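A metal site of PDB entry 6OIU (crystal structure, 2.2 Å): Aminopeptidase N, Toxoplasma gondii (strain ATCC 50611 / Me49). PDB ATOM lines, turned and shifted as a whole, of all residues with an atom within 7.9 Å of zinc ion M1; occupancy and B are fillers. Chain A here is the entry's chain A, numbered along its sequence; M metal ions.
Zinc ion M1 is bound by the side-chain carboxylate (OE2) of Glu 340 (2.0 Å), a ring nitrogen (NE2) of His 321 (2.1 Å) and a ring nitrogen (NE2) of His 317 (2.1 Å).
ND1 of His 317 sits at hydrogen-bond distance from OD1 of Asp 347 (2.8 Å). The side-chain carboxylate (OE2) of Glu 340 sits close to the side-chain hydroxyl (OH) of Tyr 401 (3.3 Å). The side-chain hydroxyl (OG1) of Thr 343 is in hydrogen-bond range of a ring nitrogen (ND1) of His 321, at 3.2 Å. The backbone carbonyl oxygen (O) of Thr 324 lies within hydrogen-bond range of a ring nitrogen (ND1) of His 321, 2.9 Å away. OE1 of Glu 340 is in salt-bridge range of NZ of Lys 339 (2.7 Å).
Tyr 401 touches zinc ion M1. The nearest printed residue that does not touch zinc ion M1 is Glu 284 (4.5 Å).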
ATOM      1  N   GLU A 139     -20.613   8.019  19.783  1.00  0.00           N
ATOM      2  CA  GLU A 139     -21.036   6.779  19.138  1.00  0.00           C
ATOM      3  C   GLU A 139     -21.267   5.703  20.194  1.00  0.00           C
ATOM      4  O   GLU A 139     -20.388   5.436  21.018  1.00  0.00           O
ATOM      5  CB  GLU A 139     -20.002   6.317  18.122  1.00  0.00           C
ATOM      6  CG  GLU A 139     -20.272   4.926  17.562  1.00  0.00           C
ATOM      7  CD  GLU A 139     -19.567   4.655  16.240  1.00  0.00           C
ATOM      8  OE1 GLU A 139     -20.237   4.184  15.298  1.00  0.00           O
ATOM      9  OE2 GLU A 139     -18.341   4.879  16.152  1.00  0.00           O
ATOM     10  N   MET A 280     -13.382   2.627  23.772  1.00  0.00           N
ATOM     11  CA  MET A 280     -12.968   2.019  22.526  1.00  0.00           C
ATOM     12  C   MET A 280     -11.456   2.097  22.366  1.00  0.00           C
ATOM     13  O   MET A 280     -10.724   2.537  23.260  1.00  0.00           O
ATOM     14  CB  MET A 280     -13.654   2.715  21.344  1.00  0.00           C
ATOM     15  CG  MET A 280     -15.172   2.735  21.412  1.00  0.00           C
ATOM     16  SD  MET A 280     -15.887   3.825  20.171  1.00  0.00           S
ATOM     17  CE  MET A 280     -15.435   2.968  18.662  1.00  0.00           C
ATOM     18  N   ALA A 282     -10.274   3.664  19.452  1.00  0.00           N
ATOM     19  CA  ALA A 282     -10.225   4.982  18.843  1.00  0.00           C
ATOM     20  C   ALA A 282     -11.587   5.289  18.251  1.00  0.00           C
ATOM     21  O   ALA A 282     -12.397   4.392  18.005  1.00  0.00           O
ATOM     22  CB  ALA A 282      -9.127   5.074  17.780  1.00  0.00           C
ATOM     23  N   MET A 283     -11.829   6.577  18.015  1.00  0.00           N
ATOM     24  CA  MET A 283     -13.100   7.047  17.470  1.00  0.00           C
ATOM     25  C   MET A 283     -12.826   8.012  16.326  1.00  0.00           C
ATOM     26  O   MET A 283     -11.899   8.819  16.384  1.00  0.00           O
ATOM     27  CB  MET A 283     -13.939   7.731  18.559  1.00  0.00           C
ATOM     28  CG  MET A 283     -15.285   8.255  18.077  1.00  0.00           C
ATOM     29  SD  MET A 283     -16.329   6.964  17.371  1.00  0.00           S
ATOM     30  CE  MET A 283     -17.303   7.922  16.210  1.00  0.00           C
ATOM     31  N   GLU A 284     -13.646   7.918  15.282  1.00  0.00           N
ATOM     32  CA  GLU A 284     -13.398   8.600  14.006  1.00  0.00           C
ATOM     33  C   GLU A 284     -14.135   9.925  13.887  1.00  0.00           C
ATOM     34  O   GLU A 284     -14.576  10.307  12.795  1.00  0.00           O
ATOM     35  CB  GLU A 284     -13.771   7.682  12.845  1.00  0.00           C
ATOM     36  CG  GLU A 284     -15.269   7.421  12.672  1.00  0.00           C
ATOM     37  CD  GLU A 284     -15.749   6.170  13.379  1.00  0.00           C
ATOM     38  OE1 GLU A 284     -15.068   5.729  14.325  1.00  0.00           O
ATOM     39  OE2 GLU A 284     -16.813   5.645  12.988  1.00  0.00           O
ATOM     40  N   VAL A 314      -4.661   0.775  13.535  1.00  0.00           N
ATOM     41  CA  VAL A 314      -5.815   1.519  14.026  1.00  0.00           C
ATOM     42  C   VAL A 314      -5.805   2.949  13.514  1.00  0.00           C
ATOM     43  O   VAL A 314      -6.860   3.521  13.206  1.00  0.00           O
ATOM     44  CB  VAL A 314      -5.877   1.442  15.560  1.00  0.00           C
ATOM     45  CG1 VAL A 314      -7.005   2.324  16.095  1.00  0.00           C
ATOM     46  CG2 VAL A 314      -6.070   0.004  16.011  1.00  0.00           C
ATOM     47  N   HIS A 317      -7.165   2.672  10.223  1.00  0.00           N
ATOM     48  CA  HIS A 317      -8.590   2.364  10.339  1.00  0.00           C
ATOM     49  C   HIS A 317      -9.420   3.624  10.573  1.00  0.00           C
ATOM     50  O   HIS A 317     -10.479   3.796   9.966  1.00  0.00           O
ATOM     51  CB  HIS A 317      -8.806   1.367  11.481  1.00  0.00           C
ATOM     52  CG  HIS A 317     -10.250   1.054  11.748  1.00  0.00           C
ATOM     53  ND1 HIS A 317     -10.862  -0.099  11.290  1.00  0.00           N
ATOM     54  CD2 HIS A 317     -11.201   1.733  12.438  1.00  0.00           C
ATOM     55  CE1 HIS A 317     -12.125  -0.112  11.685  1.00  0.00           C
ATOM     56  NE2 HIS A 317     -12.355   0.984  12.378  1.00  0.00           N
ATOM     57  N   GLU A 318      -8.940   4.512  11.436  1.00  0.00           N
ATOM     58  CA  GLU A 318      -9.719   5.712  11.750  1.00  0.00           C
ATOM     59  C   GLU A 318      -9.728   6.685  10.578  1.00  0.00           C
ATOM     60  O   GLU A 318     -10.749   7.346  10.326  1.00  0.00           O
ATOM     61  CB  GLU A 318      -9.170   6.379  13.005  1.00  0.00           C
ATOM     62  CG  GLU A 318      -9.211   5.494  14.237  1.00  0.00           C
ATOM     63  CD  GLU A 318     -10.604   4.975  14.551  1.00  0.00           C
ATOM     64  OE1 GLU A 318     -11.577   5.733  14.369  1.00  0.00           O
ATOM     65  OE2 GLU A 318     -10.713   3.824  14.999  1.00  0.00           O
ATOM     66  N   PHE A 320      -9.479   5.802   7.397  1.00  0.00           N
ATOM     67  CA  PHE A 320     -10.306   5.196   6.359  1.00  0.00           C
ATOM     68  C   PHE A 320     -11.801   5.386   6.635  1.00  0.00           C
ATOM     69  O   PHE A 320     -12.601   5.330   5.700  1.00  0.00           O
ATOM     70  CB  PHE A 320      -9.984   3.709   6.224  1.00  0.00           C
ATOM     71  CG  PHE A 320      -8.543   3.426   5.903  1.00  0.00           C
ATOM     72  CD1 PHE A 320      -7.776   4.362   5.222  1.00  0.00           C
ATOM     73  CD2 PHE A 320      -7.947   2.235   6.271  1.00  0.00           C
ATOM     74  CE1 PHE A 320      -6.456   4.110   4.919  1.00  0.00           C
ATOM     75  CE2 PHE A 320      -6.629   1.977   5.981  1.00  0.00           C
ATOM     76  CZ  PHE A 320      -5.875   2.914   5.306  1.00  0.00           C
ATOM     77  N   HIS A 321     -12.170   5.622   7.899  1.00  0.00           N
ATOM     78  CA  HIS A 321     -13.561   5.903   8.232  1.00  0.00           C
ATOM     79  C   HIS A 321     -14.042   7.229   7.649  1.00  0.00           C
ATOM     80  O   HIS A 321     -15.254   7.432   7.535  1.00  0.00           O
ATOM     81  CB  HIS A 321     -13.740   5.932   9.755  1.00  0.00           C
ATOM     82  CG  HIS A 321     -14.320   4.680  10.321  1.00  0.00           C
ATOM     83  ND1 HIS A 321     -15.359   3.998   9.723  1.00  0.00           N
ATOM     84  CD2 HIS A 321     -14.010   3.982  11.439  1.00  0.00           C
ATOM     85  CE1 HIS A 321     -15.664   2.929  10.448  1.00  0.00           C
ATOM     86  NE2 HIS A 321     -14.861   2.904  11.498  1.00  0.00           N
ATOM     87  N   THR A 324     -15.416   5.682   4.323  1.00  0.00           N
ATOM     88  CA  THR A 324     -16.287   4.563   4.668  1.00  0.00           C
ATOM     89  C   THR A 324     -16.741   4.696   6.120  1.00  0.00           C
ATOM     90  O   THR A 324     -16.300   3.988   7.027  1.00  0.00           O
ATOM     91  CB  THR A 324     -15.574   3.231   4.414  1.00  0.00           C
ATOM     92  OG1 THR A 324     -14.395   3.158   5.235  1.00  0.00           O
ATOM     93  CG2 THR A 324     -15.176   3.108   2.954  1.00  0.00           C
ATOM     94  N   GLY A 325     -17.657   5.638   6.327  1.00  0.00           N
ATOM     95  CA  GLY A 325     -18.203   5.891   7.646  1.00  0.00           C
ATOM     96  C   GLY A 325     -18.679   7.303   7.855  1.00  0.00           C
ATOM     97  O   GLY A 325     -19.732   7.525   8.459  1.00  0.00           O
ATOM     98  N   LEU A 336     -24.346  -1.166  10.967  1.00  0.00           N
ATOM     99  CA  LEU A 336     -23.046  -0.825  11.518  1.00  0.00           C
ATOM    100  C   LEU A 336     -21.916  -1.483  10.736  1.00  0.00           C
ATOM    101  O   LEU A 336     -20.856  -0.889  10.531  1.00  0.00           O
ATOM    102  CB  LEU A 336     -22.969  -1.231  12.992  1.00  0.00           C
ATOM    103  CG  LEU A 336     -21.635  -0.928  13.684  1.00  0.00           C
ATOM    104  CD1 LEU A 336     -21.376   0.565  13.693  1.00  0.00           C
ATOM    105  CD2 LEU A 336     -21.611  -1.501  15.095  1.00  0.00           C
ATOM    106  N   LYS A 339     -20.010   0.248   7.577  1.00  0.00           N
ATOM    107  CA  LYS A 339     -18.770   1.010   7.741  1.00  0.00           C
ATOM    108  C   LYS A 339     -17.708   0.263   8.518  1.00  0.00           C
ATOM    109  O   LYS A 339     -16.522   0.465   8.253  1.00  0.00           O
ATOM    110  CB  LYS A 339     -19.057   2.364   8.418  1.00  0.00           C
ATOM    111  CG  LYS A 339     -19.403   2.300   9.902  1.00  0.00           C
ATOM    112  CD  LYS A 339     -19.663   3.702  10.432  1.00  0.00           C
ATOM    113  CE  LYS A 339     -20.172   3.693  11.864  1.00  0.00           C
ATOM    114  NZ  LYS A 339     -19.060   3.650  12.865  1.00  0.00           N
ATOM    115  N   GLU A 340     -18.089  -0.600   9.461  1.00  0.00           N
ATOM    116  CA  GLU A 340     -17.070  -1.284  10.264  1.00  0.00           C
ATOM    117  C   GLU A 340     -16.440  -2.441   9.509  1.00  0.00           C
ATOM    118  O   GLU A 340     -15.215  -2.587   9.492  1.00  0.00           O
ATOM    119  CB  GLU A 340     -17.672  -1.761  11.584  1.00  0.00           C
ATOM    120  CG  GLU A 340     -18.090  -0.634  12.533  1.00  0.00           C
ATOM    121  CD  GLU A 340     -16.998   0.399  12.754  1.00  0.00           C
ATOM    122  OE1 GLU A 340     -17.341   1.581  12.953  1.00  0.00           O
ATOM    123  OE2 GLU A 340     -15.806   0.034  12.734  1.00  0.00           O
ATOM    124  N   GLY A 341     -17.262  -3.283   8.881  1.00  0.00           N
ATOM    125  CA  GLY A 341     -16.707  -4.388   8.100  1.00  0.00           C
ATOM    126  C   GLY A 341     -15.893  -3.903   6.927  1.00  0.00           C
ATOM    127  O   GLY A 341     -14.858  -4.496   6.588  1.00  0.00           O
ATOM    128  N   THR A 343     -14.327  -0.911   6.679  1.00  0.00           N
ATOM    129  CA  THR A 343     -13.126  -0.218   7.128  1.00  0.00           C
ATOM    130  C   THR A 343     -12.099  -1.173   7.716  1.00  0.00           C
ATOM    131  O   THR A 343     -10.892  -0.956   7.550  1.00  0.00           O
ATOM    132  CB  THR A 343     -13.496   0.862   8.146  1.00  0.00           C
ATOM    133  OG1 THR A 343     -14.450   1.770   7.561  1.00  0.00           O
ATOM    134  CG2 THR A 343     -12.267   1.650   8.565  1.00  0.00           C
ATOM    135  N   VAL A 344     -12.553  -2.229   8.398  1.00  0.00           N
ATOM    136  CA  VAL A 344     -11.604  -3.223   8.904  1.00  0.00           C
ATOM    137  C   VAL A 344     -10.898  -3.913   7.742  1.00  0.00           C
ATOM    138  O   VAL A 344      -9.674  -4.111   7.773  1.00  0.00           O
ATOM    139  CB  VAL A 344     -12.311  -4.240   9.815  1.00  0.00           C
ATOM    140  CG1 VAL A 344     -11.401  -5.424  10.100  1.00  0.00           C
ATOM    141  CG2 VAL A 344     -12.717  -3.577  11.120  1.00  0.00           C
ATOM    142  N   ASP A 347      -8.232  -1.538   6.524  1.00  0.00           N
ATOM    143  CA  ASP A 347      -7.008  -1.503   7.317  1.00  0.00           C
ATOM    144  C   ASP A 347      -6.251  -2.827   7.251  1.00  0.00           C
ATOM    145  O   ASP A 347      -5.047  -2.849   7.531  1.00  0.00           O
ATOM    146  CB  ASP A 347      -7.306  -1.109   8.779  1.00  0.00           C
ATOM    147  CG  ASP A 347      -8.019  -2.202   9.568  1.00  0.00           C
ATOM    148  OD1 ASP A 347      -9.095  -1.905  10.121  1.00  0.00           O
ATOM    149  OD2 ASP A 347      -7.500  -3.334   9.692  1.00  0.00           O
ATOM    150  N   TYR A 396     -20.965  -3.930  18.917  1.00  0.00           N
ATOM    151  CA  TYR A 396     -19.669  -3.573  18.351  1.00  0.00           C
ATOM    152  C   TYR A 396     -18.721  -4.746  18.562  1.00  0.00           C
ATOM    153  O   TYR A 396     -17.791  -4.725  19.377  1.00  0.00           O
ATOM    154  CB  TYR A 396     -19.154  -2.278  18.962  1.00  0.00           C
ATOM    155  CG  TYR A 396     -19.881  -1.049  18.462  1.00  0.00           C
ATOM    156  CD1 TYR A 396     -21.200  -0.821  18.810  1.00  0.00           C
ATOM    157  CD2 TYR A 396     -19.245  -0.125  17.643  1.00  0.00           C
ATOM    158  CE1 TYR A 396     -21.875   0.295  18.350  1.00  0.00           C
ATOM    159  CE2 TYR A 396     -19.914   0.983  17.181  1.00  0.00           C
ATOM    160  CZ  TYR A 396     -21.224   1.190  17.538  1.00  0.00           C
ATOM    161  OH  TYR A 396     -21.896   2.307  17.087  1.00  0.00           O
ATOM    162  N   TYR A 401     -17.439  -6.484  13.143  1.00  0.00           N
ATOM    163  CA  TYR A 401     -16.165  -5.906  12.703  1.00  0.00           C
ATOM    164  C   TYR A 401     -15.396  -6.865  11.806  1.00  0.00           C
ATOM    165  O   TYR A 401     -15.156  -6.579  10.628  1.00  0.00           O
ATOM    166  CB  TYR A 401     -15.319  -5.527  13.912  1.00  0.00           C
ATOM    167  CG  TYR A 401     -15.576  -4.153  14.454  1.00  0.00           C
ATOM    168  CD1 TYR A 401     -16.783  -3.833  15.075  1.00  0.00           C
ATOM    169  CD2 TYR A 401     -14.610  -3.157  14.361  1.00  0.00           C
ATOM    170  CE1 TYR A 401     -17.018  -2.572  15.572  1.00  0.00           C
ATOM    171  CE2 TYR A 401     -14.838  -1.889  14.854  1.00  0.00           C
ATOM    172  CZ  TYR A 401     -16.038  -1.600  15.463  1.00  0.00           C
ATOM    173  OH  TYR A 401     -16.266  -0.332  15.956  1.00  0.00           O
HETATM  174 ZN    ZN M   1     -14.373   1.475  12.907  1.00  0.00          ZN
HETATM  175 ZN    ZN M   2     -13.949   2.315  15.027  1.00  0.00          ZN
